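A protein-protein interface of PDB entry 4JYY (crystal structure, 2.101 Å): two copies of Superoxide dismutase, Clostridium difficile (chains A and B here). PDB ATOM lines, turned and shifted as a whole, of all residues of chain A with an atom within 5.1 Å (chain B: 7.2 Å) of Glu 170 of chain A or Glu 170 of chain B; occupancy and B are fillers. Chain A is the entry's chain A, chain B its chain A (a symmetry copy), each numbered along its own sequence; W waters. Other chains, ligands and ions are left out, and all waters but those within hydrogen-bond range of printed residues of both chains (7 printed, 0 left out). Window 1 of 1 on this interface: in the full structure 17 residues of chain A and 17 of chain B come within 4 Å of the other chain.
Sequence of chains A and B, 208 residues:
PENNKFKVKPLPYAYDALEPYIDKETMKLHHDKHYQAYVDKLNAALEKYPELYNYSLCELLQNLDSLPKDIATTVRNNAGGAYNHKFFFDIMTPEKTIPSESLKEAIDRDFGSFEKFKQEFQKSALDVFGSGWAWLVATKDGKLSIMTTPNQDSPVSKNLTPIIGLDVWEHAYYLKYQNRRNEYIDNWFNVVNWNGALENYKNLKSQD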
ATOM      1  N   HIS A  34     -27.742   8.831  -6.943  1.00  0.00           N
ATOM      2  CA  HIS A  34     -27.968   7.403  -7.142  1.00  0.00           C
ATOM      3  C   HIS A  34     -29.465   7.051  -7.173  1.00  0.00           C
ATOM      4  O   HIS A  34     -29.962   6.471  -8.134  1.00  0.00           O
ATOM      5  CB  HIS A  34     -27.244   6.596  -6.057  1.00  0.00           C
ATOM      6  CG  HIS A  34     -25.749   6.707  -6.123  1.00  0.00           C
ATOM      7  ND1 HIS A  34     -24.987   5.981  -7.017  1.00  0.00           N
ATOM      8  CD2 HIS A  34     -24.882   7.473  -5.424  1.00  0.00           C
ATOM      9  CE1 HIS A  34     -23.712   6.280  -6.848  1.00  0.00           C
ATOM     10  NE2 HIS A  34     -23.617   7.184  -5.889  1.00  0.00           N
ATOM     11  N   SER A 131     -21.445  -5.575  -4.635  1.00  0.00           N
ATOM     12  CA  SER A 131     -22.513  -4.662  -4.247  1.00  0.00           C
ATOM     13  C   SER A 131     -23.734  -5.428  -3.759  1.00  0.00           C
ATOM     14  O   SER A 131     -24.051  -6.497  -4.285  1.00  0.00           O
ATOM     15  CB  SER A 131     -22.917  -3.793  -5.440  1.00  0.00           C
ATOM     16  OG  SER A 131     -21.788  -3.109  -5.977  1.00  0.00           O
ATOM     17  N   VAL A 168     -25.041  -1.923   1.414  1.00  0.00           N
ATOM     18  CA  VAL A 168     -23.575  -2.019   1.493  1.00  0.00           C
ATOM     19  C   VAL A 168     -22.852  -1.905   0.143  1.00  0.00           C
ATOM     20  O   VAL A 168     -21.718  -2.365   0.000  1.00  0.00           O
ATOM     21  CB  VAL A 168     -23.074  -3.257   2.287  1.00  0.00           C
ATOM     22  CG1 VAL A 168     -23.472  -3.148   3.762  1.00  0.00           C
ATOM     23  CG2 VAL A 168     -23.591  -4.561   1.657  1.00  0.00           C
ATOM     24  N   TRP A 169     -23.505  -1.299  -0.840  1.00  0.00           N
ATOM     25  CA  TRP A 169     -22.785  -0.789  -1.995  1.00  0.00           C
ATOM     26  C   TRP A 169     -21.742   0.186  -1.447  1.00  0.00           C
ATOM     27  O   TRP A 169     -21.996   0.904  -0.461  1.00  0.00           O
ATOM     28  CB  TRP A 169     -23.709  -0.023  -2.932  1.00  0.00           C
ATOM     29  CG  TRP A 169     -24.614  -0.853  -3.806  1.00  0.00           C
ATOM     30  CD1 TRP A 169     -25.536  -1.783  -3.399  1.00  0.00           C
ATOM     31  CD2 TRP A 169     -24.715  -0.788  -5.240  1.00  0.00           C
ATOM     32  NE1 TRP A 169     -26.191  -2.302  -4.492  1.00  0.00           N
ATOM     33  CE2 TRP A 169     -25.710  -1.708  -5.631  1.00  0.00           C
ATOM     34  CE3 TRP A 169     -24.070  -0.031  -6.226  1.00  0.00           C
ATOM     35  CZ2 TRP A 169     -26.064  -1.906  -6.972  1.00  0.00           C
ATOM     36  CZ3 TRP A 169     -24.415  -0.230  -7.553  1.00  0.00           C
ATOM     37  CH2 TRP A 169     -25.412  -1.163  -7.915  1.00  0.00           C
ATOM     38  N   GLU A 170     -20.577   0.223  -2.082  1.00  0.00           N
ATOM     39  CA  GLU A 170     -19.505   1.091  -1.614  1.00  0.00           C
ATOM     40  C   GLU A 170     -19.887   2.571  -1.659  1.00  0.00           C
ATOM     41  O   GLU A 170     -19.446   3.321  -0.819  1.00  0.00           O
ATOM     42  CB  GLU A 170     -18.176   0.785  -2.343  1.00  0.00           C
ATOM     43  CG  GLU A 170     -17.566  -0.534  -1.860  1.00  0.00           C
ATOM     44  CD  GLU A 170     -16.394  -1.033  -2.703  1.00  0.00           C
ATOM     45  OE1 GLU A 170     -16.397  -0.816  -3.920  1.00  0.00           O
ATOM     46  OE2 GLU A 170     -15.481  -1.654  -2.131  1.00  0.00           O
ATOM     47  N   HIS A 171     -20.732   2.989  -2.595  1.00  0.00           N
ATOM     48  CA  HIS A 171     -21.142   4.391  -2.589  1.00  0.00           C
ATOM     49  C   HIS A 171     -21.852   4.810  -1.297  1.00  0.00           C
ATOM     50  O   HIS A 171     -21.926   6.000  -0.989  1.00  0.00           O
ATOM     51  CB  HIS A 171     -21.979   4.771  -3.817  1.00  0.00           C
ATOM     52  CG  HIS A 171     -23.313   4.090  -3.887  1.00  0.00           C
ATOM     53  ND1 HIS A 171     -23.727   3.373  -4.995  1.00  0.00           N
ATOM     54  CD2 HIS A 171     -24.338   4.039  -3.003  1.00  0.00           C
ATOM     55  CE1 HIS A 171     -24.947   2.908  -4.783  1.00  0.00           C
ATOM     56  NE2 HIS A 171     -25.334   3.290  -3.580  1.00  0.00           N
ATOM     57  N   ALA A 172     -22.356   3.840  -0.541  1.00  0.00           N
ATOM     58  CA  ALA A 172     -23.097   4.142   0.681  1.00  0.00           C
ATOM     59  C   ALA A 172     -22.172   4.504   1.830  1.00  0.00           C
ATOM     60  O   ALA A 172     -22.614   5.095   2.815  1.00  0.00           O
ATOM     61  CB  ALA A 172     -24.000   2.964   1.090  1.00  0.00           C
ATOM     62  N   TYR A 173     -20.897   4.144   1.720  1.00  0.00           N
ATOM     63  CA  TYR A 173     -20.008   4.343   2.851  1.00  0.00           C
ATOM     64  C   TYR A 173     -18.577   4.757   2.542  1.00  0.00           C
ATOM     65  O   TYR A 173     -17.811   4.994   3.467  1.00  0.00           O
ATOM     66  CB  TYR A 173     -19.976   3.090   3.723  1.00  0.00           C
ATOM     67  CG  TYR A 173     -19.416   1.832   3.063  1.00  0.00           C
ATOM     68  CD1 TYR A 173     -18.049   1.574   3.050  1.00  0.00           C
ATOM     69  CD2 TYR A 173     -20.262   0.885   2.481  1.00  0.00           C
ATOM     70  CE1 TYR A 173     -17.534   0.388   2.477  1.00  0.00           C
ATOM     71  CE2 TYR A 173     -19.753  -0.299   1.903  1.00  0.00           C
ATOM     72  CZ  TYR A 173     -18.399  -0.539   1.902  1.00  0.00           C
ATOM     73  OH  TYR A 173     -17.895  -1.712   1.337  1.00  0.00           O
ATOM     74  N   TYR A 174     -18.190   4.818   1.273  1.00  0.00           N
ATOM     75  CA  TYR A 174     -16.755   4.985   0.976  1.00  0.00           C
ATOM     76  C   TYR A 174     -16.178   6.365   1.375  1.00  0.00           C
ATOM     77  O   TYR A 174     -15.059   6.444   1.863  1.00  0.00           O
ATOM     78  CB  TYR A 174     -16.416   4.661  -0.495  1.00  0.00           C
ATOM     79  CG  TYR A 174     -15.070   3.969  -0.603  1.00  0.00           C
ATOM     80  CD1 TYR A 174     -14.918   2.644  -0.204  1.00  0.00           C
ATOM     81  CD2 TYR A 174     -13.943   4.646  -1.064  1.00  0.00           C
ATOM     82  CE1 TYR A 174     -13.679   2.001  -0.260  1.00  0.00           C
ATOM     83  CE2 TYR A 174     -12.696   4.010  -1.130  1.00  0.00           C
ATOM     84  CZ  TYR A 174     -12.571   2.696  -0.730  1.00  0.00           C
ATOM     85  OH  TYR A 174     -11.343   2.064  -0.784  1.00  0.00           O
ATOM     86  N   THR B  26      -6.636   6.960  -3.053  1.00  0.00           N
ATOM     87  CA  THR B  26      -7.297   5.788  -3.640  1.00  0.00           C
ATOM     88  C   THR B  26      -6.277   4.701  -3.994  1.00  0.00           C
ATOM     89  O   THR B  26      -6.487   3.521  -3.690  1.00  0.00           O
ATOM     90  CB  THR B  26      -8.154   6.185  -4.867  1.00  0.00           C
ATOM     91  OG1 THR B  26      -9.302   6.903  -4.404  1.00  0.00           O
ATOM     92  CG2 THR B  26      -8.623   4.940  -5.676  1.00  0.00           C
ATOM     93  N   HIS B  34      -7.503  -3.123  -0.244  1.00  0.00           N
ATOM     94  CA  HIS B  34      -8.341  -4.039  -1.013  1.00  0.00           C
ATOM     95  C   HIS B  34      -7.533  -5.204  -1.607  1.00  0.00           C
ATOM     96  O   HIS B  34      -7.829  -6.371  -1.366  1.00  0.00           O
ATOM     97  CB  HIS B  34      -9.085  -3.277  -2.115  1.00  0.00           C
ATOM     98  CG  HIS B  34     -10.076  -2.279  -1.592  1.00  0.00           C
ATOM     99  ND1 HIS B  34     -11.332  -2.641  -1.147  1.00  0.00           N
ATOM    100  CD2 HIS B  34      -9.988  -0.939  -1.423  1.00  0.00           C
ATOM    101  CE1 HIS B  34     -11.982  -1.563  -0.748  1.00  0.00           C
ATOM    102  NE2 HIS B  34     -11.191  -0.516  -0.903  1.00  0.00           N
ATOM    103  N   TYR B  38      -7.607  -9.425  -0.519  1.00  0.00           N
ATOM    104  CA  TYR B  38      -7.827 -10.577  -1.391  1.00  0.00           C
ATOM    105  C   TYR B  38      -6.732 -11.619  -1.213  1.00  0.00           C
ATOM    106  O   TYR B  38      -7.011 -12.808  -1.086  1.00  0.00           O
ATOM    107  CB  TYR B  38      -7.928 -10.153  -2.855  1.00  0.00           C
ATOM    108  CG  TYR B  38      -9.177  -9.349  -3.143  1.00  0.00           C
ATOM    109  CD1 TYR B  38     -10.442  -9.834  -2.791  1.00  0.00           C
ATOM    110  CD2 TYR B  38      -9.094  -8.105  -3.758  1.00  0.00           C
ATOM    111  CE1 TYR B  38     -11.599  -9.092  -3.058  1.00  0.00           C
ATOM    112  CE2 TYR B  38     -10.232  -7.362  -4.029  1.00  0.00           C
ATOM    113  CZ  TYR B  38     -11.482  -7.856  -3.667  1.00  0.00           C
ATOM    114  OH  TYR B  38     -12.606  -7.107  -3.955  1.00  0.00           O
ATOM    115  N   GLY B 130     -23.600  -2.697 -10.661  1.00  0.00           N
ATOM    116  CA  GLY B 130     -22.974  -3.221  -9.463  1.00  0.00           C
ATOM    117  C   GLY B 130     -21.466  -3.210  -9.605  1.00  0.00           C
ATOM    118  O   GLY B 130     -20.920  -2.394 -10.340  1.00  0.00           O
ATOM    119  N   SER B 131     -20.792  -4.113  -8.901  1.00  0.00           N
ATOM    120  CA  SER B 131     -19.335  -4.171  -8.937  1.00  0.00           C
ATOM    121  C   SER B 131     -18.852  -5.032 -10.095  1.00  0.00           C
ATOM    122  O   SER B 131     -19.480  -6.041 -10.426  1.00  0.00           O
ATOM    123  CB  SER B 131     -18.803  -4.759  -7.627  1.00  0.00           C
ATOM    124  OG  SER B 131     -19.289  -4.025  -6.506  1.00  0.00           O
ATOM    125  N   GLY B 132     -17.736  -4.639 -10.705  1.00  0.00           N
ATOM    126  CA  GLY B 132     -17.137  -5.454 -11.748  1.00  0.00           C
ATOM    127  C   GLY B 132     -16.031  -4.779 -12.545  1.00  0.00           C
ATOM    128  O   GLY B 132     -15.463  -3.765 -12.123  1.00  0.00           O
ATOM    129  N   ASP B 167     -11.077  -1.612 -13.559  1.00  0.00           N
ATOM    130  CA  ASP B 167     -11.850  -1.876 -12.350  1.00  0.00           C
ATOM    131  C   ASP B 167     -12.937  -0.815 -12.215  1.00  0.00           C
ATOM    132  O   ASP B 167     -12.617   0.368 -12.084  1.00  0.00           O
ATOM    133  CB  ASP B 167     -10.901  -1.765 -11.157  1.00  0.00           C
ATOM    134  CG  ASP B 167     -11.518  -2.214  -9.856  1.00  0.00           C
ATOM    135  OD1 ASP B 167     -12.750  -2.443  -9.776  1.00  0.00           O
ATOM    136  OD2 ASP B 167     -10.750  -2.341  -8.886  1.00  0.00           O
ATOM    137  N   VAL B 168     -14.216  -1.207 -12.246  1.00  0.00           N
ATOM    138  CA  VAL B 168     -15.285  -0.234 -11.964  1.00  0.00           C
ATOM    139  C   VAL B 168     -16.084  -0.515 -10.683  1.00  0.00           C
ATOM    140  O   VAL B 168     -17.220  -0.061 -10.541  1.00  0.00           O
ATOM    141  CB  VAL B 168     -16.237   0.011 -13.166  1.00  0.00           C
ATOM    142  CG1 VAL B 168     -15.485   0.682 -14.321  1.00  0.00           C
ATOM    143  CG2 VAL B 168     -16.907  -1.299 -13.615  1.00  0.00           C
ATOM    144  N   TRP B 169     -15.494  -1.260  -9.757  1.00  0.00           N
ATOM    145  CA  TRP B 169     -15.976  -1.247  -8.385  1.00  0.00           C
ATOM    146  C   TRP B 169     -15.913   0.213  -7.930  1.00  0.00           C
ATOM    147  O   TRP B 169     -14.994   0.961  -8.311  1.00  0.00           O
ATOM    148  CB  TRP B 169     -15.078  -2.070  -7.472  1.00  0.00           C
ATOM    149  CG  TRP B 169     -15.230  -3.568  -7.558  1.00  0.00           C
ATOM    150  CD1 TRP B 169     -15.087  -4.353  -8.673  1.00  0.00           C
ATOM    151  CD2 TRP B 169     -15.507  -4.464  -6.467  1.00  0.00           C
ATOM    152  NE1 TRP B 169     -15.269  -5.677  -8.339  1.00  0.00           N
ATOM    153  CE2 TRP B 169     -15.523  -5.771  -6.994  1.00  0.00           C
ATOM    154  CE3 TRP B 169     -15.727  -4.286  -5.096  1.00  0.00           C
ATOM    155  CZ2 TRP B 169     -15.771  -6.899  -6.199  1.00  0.00           C
ATOM    156  CZ3 TRP B 169     -15.978  -5.399  -4.310  1.00  0.00           C
ATOM    157  CH2 TRP B 169     -15.993  -6.697  -4.867  1.00  0.00           C
ATOM    158  N   GLU B 170     -16.878   0.617  -7.112  1.00  0.00           N
ATOM    159  CA  GLU B 170     -16.928   1.999  -6.653  1.00  0.00           C
ATOM    160  C   GLU B 170     -15.696   2.391  -5.836  1.00  0.00           C
ATOM    161  O   GLU B 170     -15.281   3.525  -5.899  1.00  0.00           O
ATOM    162  CB  GLU B 170     -18.259   2.301  -5.926  1.00  0.00           C
ATOM    163  CG  GLU B 170     -19.426   2.395  -6.914  1.00  0.00           C
ATOM    164  CD  GLU B 170     -20.805   2.437  -6.260  1.00  0.00           C
ATOM    165  OE1 GLU B 170     -20.991   1.803  -5.214  1.00  0.00           O
ATOM    166  OE2 GLU B 170     -21.699   3.101  -6.814  1.00  0.00           O
ATOM    167  N   HIS B 171     -15.083   1.462  -5.111  1.00  0.00           N
ATOM    168  CA  HIS B 171     -13.870   1.830  -4.387  1.00  0.00           C
ATOM    169  C   HIS B 171     -12.744   2.326  -5.303  1.00  0.00           C
ATOM    170  O   HIS B 171     -11.823   3.001  -4.841  1.00  0.00           O
ATOM    171  CB  HIS B 171     -13.366   0.714  -3.463  1.00  0.00           C
ATOM    172  CG  HIS B 171     -12.901  -0.518  -4.180  1.00  0.00           C
ATOM    173  ND1 HIS B 171     -13.386  -1.780  -3.889  1.00  0.00           N
ATOM    174  CD2 HIS B 171     -11.977  -0.688  -5.156  1.00  0.00           C
ATOM    175  CE1 HIS B 171     -12.781  -2.668  -4.659  1.00  0.00           C
ATOM    176  NE2 HIS B 171     -11.930  -2.029  -5.442  1.00  0.00           N
ATOM    177  N   ALA B 172     -12.825   2.007  -6.589  1.00  0.00           N
ATOM    178  CA  ALA B 172     -11.775   2.387  -7.530  1.00  0.00           C
ATOM    179  C   ALA B 172     -11.871   3.850  -7.926  1.00  0.00           C
ATOM    180  O   ALA B 172     -10.904   4.416  -8.434  1.00  0.00           O
ATOM    181  CB  ALA B 172     -11.808   1.502  -8.790  1.00  0.00           C
ATOM    182  N   TYR B 173     -13.031   4.461  -7.713  1.00  0.00           N
ATOM    183  CA  TYR B 173     -13.215   5.816  -8.203  1.00  0.00           C
ATOM    184  C   TYR B 173     -14.029   6.763  -7.333  1.00  0.00           C
ATOM    185  O   TYR B 173     -14.156   7.930  -7.678  1.00  0.00           O
ATOM    186  CB  TYR B 173     -13.828   5.792  -9.601  1.00  0.00           C
ATOM    187  CG  TYR B 173     -15.229   5.196  -9.706  1.00  0.00           C
ATOM    188  CD1 TYR B 173     -16.360   5.973  -9.479  1.00  0.00           C
ATOM    189  CD2 TYR B 173     -15.420   3.859 -10.065  1.00  0.00           C
ATOM    190  CE1 TYR B 173     -17.660   5.432  -9.618  1.00  0.00           C
ATOM    191  CE2 TYR B 173     -16.715   3.313 -10.201  1.00  0.00           C
ATOM    192  CZ  TYR B 173     -17.822   4.097  -9.976  1.00  0.00           C
ATOM    193  OH  TYR B 173     -19.103   3.558 -10.116  1.00  0.00           O
ATOM    194  N   TYR B 174     -14.604   6.286  -6.236  1.00  0.00           N
ATOM    195  CA  TYR B 174     -15.580   7.131  -5.521  1.00  0.00           C
ATOM    196  C   TYR B 174     -14.965   8.376  -4.838  1.00  0.00           C
ATOM    197  O   TYR B 174     -15.563   9.442  -4.853  1.00  0.00           O
ATOM    198  CB  TYR B 174     -16.431   6.326  -4.515  1.00  0.00           C
ATOM    199  CG  TYR B 174     -17.859   6.835  -4.482  1.00  0.00           C
ATOM    200  CD1 TYR B 174     -18.732   6.574  -5.536  1.00  0.00           C
ATOM    201  CD2 TYR B 174     -18.327   7.610  -3.424  1.00  0.00           C
ATOM    202  CE1 TYR B 174     -20.039   7.068  -5.543  1.00  0.00           C
ATOM    203  CE2 TYR B 174     -19.639   8.105  -3.416  1.00  0.00           C
ATOM    204  CZ  TYR B 174     -20.484   7.832  -4.471  1.00  0.00           C
ATOM    205  OH  TYR B 174     -21.776   8.323  -4.474  1.00  0.00           O
ATOM    206  N   LEU B 175     -13.779   8.234  -4.256  1.00  0.00           N
ATOM    207  CA  LEU B 175     -13.158   9.363  -3.541  1.00  0.00           C
ATOM    208  C   LEU B 175     -12.994  10.571  -4.442  1.00  0.00           C
ATOM    209  O   LEU B 175     -13.318  11.687  -4.048  1.00  0.00           O
ATOM    210  CB  LEU B 175     -11.815   8.976  -2.922  1.00  0.00           C
ATOM    211  CG  LEU B 175     -11.921   7.952  -1.798  1.00  0.00           C
ATOM    212  CD1 LEU B 175     -10.567   7.768  -1.127  1.00  0.00           C
ATOM    213  CD2 LEU B 175     -12.975   8.388  -0.783  1.00  0.00           C
ATOM    214  N   GLN B 178     -16.827  10.280  -7.195  1.00  0.00           N
ATOM    215  CA  GLN B 178     -18.150   9.935  -6.663  1.00  0.00           C
ATOM    216  C   GLN B 178     -18.936   9.118  -7.695  1.00  0.00           C
ATOM    217  O   GLN B 178     -18.398   8.153  -8.234  1.00  0.00           O
ATOM    218  CB  GLN B 178     -18.913  11.186  -6.201  1.00  0.00           C
ATOM    219  CG  GLN B 178     -18.190  11.925  -5.056  1.00  0.00           C
ATOM    220  CD  GLN B 178     -17.050  12.804  -5.551  1.00  0.00           C
ATOM    221  OE1 GLN B 178     -17.244  13.637  -6.430  1.00  0.00           O
ATOM    222  NE2 GLN B 178     -15.862  12.620  -4.991  1.00  0.00           N
ATOM    223  N   ASN B 179     -20.180   9.498  -7.992  1.00  0.00           N
ATOM    224  CA  ASN B 179     -21.015   8.726  -8.917  1.00  0.00           C
ATOM    225  C   ASN B 179     -20.631   8.895 -10.378  1.00  0.00           C
ATOM    226  O   ASN B 179     -21.186   8.213 -11.250  1.00  0.00           O
ATOM    227  CB  ASN B 179     -22.473   9.148  -8.780  1.00  0.00           C
ATOM    228  CG  ASN B 179     -22.671  10.603  -9.157  1.00  0.00           C
ATOM    229  OD1 ASN B 179     -22.156  11.484  -8.485  1.00  0.00           O
ATOM    230  ND2 ASN B 179     -23.373  10.852 -10.246  1.00  0.00           N
ATOM    231  N   ARG B 181     -18.838   7.919 -12.804  1.00  0.00           N
ATOM    232  CA  ARG B 181     -17.987   6.874 -13.367  1.00  0.00           C
ATOM    233  C   ARG B 181     -17.534   7.226 -14.783  1.00  0.00           C
ATOM    234  O   ARG B 181     -16.418   6.908 -15.172  1.00  0.00           O
ATOM    235  CB  ARG B 181     -18.694   5.507 -13.369  1.00  0.00           C
ATOM    236  CG  ARG B 181     -17.741   4.326 -13.610  1.00  0.00           C
ATOM    237  CD  ARG B 181     -18.512   3.044 -14.023  1.00  0.00           C
ATOM    238  NE  ARG B 181     -19.306   2.482 -12.928  1.00  0.00           N
ATOM    239  CZ  ARG B 181     -20.125   1.434 -13.063  1.00  0.00           C
ATOM    240  NH1 ARG B 181     -20.267   0.831 -14.245  1.00  0.00           N
ATOM    241  NH2 ARG B 181     -20.808   0.988 -12.018  1.00  0.00           N
HETATM  242  O   HOH W   1     -23.383   8.032  -2.076  1.00  0.00           O
HETATM  243  O   HOH W   2     -18.269  -1.593  -5.663  1.00  0.00           O
HETATM  244  O   HOH W   3     -21.832  -6.415  -7.416  1.00  0.00           O
HETATM  245  O   HOH W   4     -20.667  -0.827  -4.877  1.00  0.00           O
HETATM  246  O   HOH W   5      -9.758   2.308  -3.202  1.00  0.00           O
HETATM  247  O   HOH W   6     -24.692   3.334  -8.354  1.00  0.00           O
HETATM  248  O   HOH W   7     -13.650  -4.447  -1.647  1.00  0.00           O
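The side-chain hydroxyl (OH) of Tyr 174 of chain A lies within hydrogen-bond range of a ring nitrogen (NE2) of His 34 of chain B (2.6 Å).
The side-chain carboxylate (OE2) of Glu 170 of chain B is in hydrogen-bond range of a ring nitrogen (ND1) of His 171 of chain A.
The side-chain hydroxyl (OH) of Tyr 174 of chain B lies within hydrogen-bond range of a ring nitrogen (NE2) of His 34 of chain A, 2.6 Å away.
The side-chain carboxylate (OE2) of Glu 170 of chain A sits at hydrogen-bond distance from a ring nitrogen (ND1) of His 171 of chain B.
The side-chain hydroxyl (OG) of Ser 131 of chain A lies within hydrogen-bond range of the side-chain hydroxyl (OG) of Ser 131 of chain B (2.7 Å).
The side-chain amide nitrogen of Gln 178 of chain B lies within hydrogen-bond range of the backbone carbonyl oxygen of Tyr 174 of chain B, 3.2 Å away.
The side-chain amide nitrogen (NE2) of Gln 178 of chain B sits at hydrogen-bond distance from the backbone carbonyl oxygen (O) of Leu 175 of chain B, at 2.9 Å.
N of Trp 169 of chain B sits at hydrogen-bond distance from O of Gly 132 of chain B (3.4 Å).
The side-chain carboxylate of Asp 167 of chain B sits at hydrogen-bond distance from the backbone NH of Trp 169 of chain B (3.0 Å).
Glu 170 of chain B touches His 34 of chain A.
Asn 179 of chain B touches His 34 of chain A (CB to CE1, 3.7 Å).
Ser 131 of chain A touches Gly 130 of chain B.
CA of Gly 130 of chain B touches CH2 of Trp 169 of chain A, at 3.5 Å.
OE1 of Glu 170 of chain B touches CE3 of Trp 169 of chain A (3.7 Å).
OE2 of Glu 170 of chain A touches CE1 of His 34 of chain B, 3.8 Å away.
Glu 170 of chain A touches Trp 169 of chain B (OE1 to CE3, 3.7 Å).
Glu 170 of chain A touches Glu 170 of chain B (OE1 to N, 3.5 Å).
Tyr 174 of chain B touches His 171 of chain A.
Tyr 174 of chain A touches His 171 of chain B (CE1 to CB, 3.5 Å).
Glu 170 of chain A touches just these residues of chain B: His 34 (3.8 Å), Trp 169 (3.7 Å), Glu 170 (3.5 Å) and His 171 (2.7 Å).
Of chain A, only His 34 (3.8 Å), Trp 169 (3.7 Å), Glu 170 (3.5 Å) and His 171 (2.7 Å) come within 4 Å of Glu 170 of chain B.
Printed residues of chain B within 4 Å of His 34 of chain A: Glu 170, Tyr 174 and Asn 179.
Of the printed residues of chain A, His 34 of chain B touches Glu 170 (3.8 Å) and Tyr 174 (2.6 Å).
Of the printed residues of chain B, Trp 169 of chain A touches Gly 130 and Glu 170.
Printed residues of chain B within 4 Å of His 171 of chain A: Glu 170 and Tyr 174.
Printed residues of chain A within 4 Å of Tyr 174 of chain B: His 34 and His 171.
The nearest residue of chain A that does not touch Glu 170 of chain B is Ser 131 of chain A (5.0 Å).
The nearest printed residue of chain A that does not touch Tyr 174 of chain B is Tyr 174 of chain A (4.4 Å).
Hydrophobic or aromatic side chains of chain B that line the printed part of chain A: His 34, Trp 169, His 171, Tyr 174 and Leu 175.
Among the printed residues, no Asp or Glu carboxylate lies within 4 Å of a Lys or Arg side-chain nitrogen of the other chain.
His 34 of chain A touches Glu 170 of chain B, and with the chains exchanged Glu 170 of chain A touches His 34 of chain B.
His 34 of chain A touches Tyr 174 of chain B, and with the chains exchanged Tyr 174 of chain A touches His 34 of chain B.
Ser 131 of chain A touches its own counterpart, Ser 131 of chain B.
Glu 170 of chain A touches His 171 of chain B, and with the chains exchanged His 171 of chain A touches Glu 170 of chain B.
Of the 16 pairs that touch across the chains among the printed residues, 12 have their exchanged pair printed and touching as well.
Water W4 lies within hydrogen-bond range of OE1 of Glu 170 of chain B (2.7 Å), OG of Ser 131 of chain A (2.8 Å) and N of Glu 170 of chain A (3.0 Å).
Water W2 lies within hydrogen-bond range of OE1 of Glu 170 of chain A, OG of Ser 131 of chain B and N of Glu 170 of chain B.
Water W1 bridges O of His 171 of chain A and OH of Tyr 174 of chain B.
Water W5 lies within hydrogen-bond range of O of His 171 of chain B (2.7 Å) and OH of Tyr 174 of chain A (2.9 Å).
Water W7 lies within hydrogen-bond range of ND1 of His 34 of chain B (3.0 Å), OE2 of Glu 170 of chain A (3.4 Å) and ND1 of His 171 of chain B (3.5 Å).
Water W6 lies within hydrogen-bond range of ND1 of His 34 of chain A (3.0 Å), OE2 of Glu 170 of chain B (3.4 Å) and ND1 of His 171 of chain A (3.5 Å).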
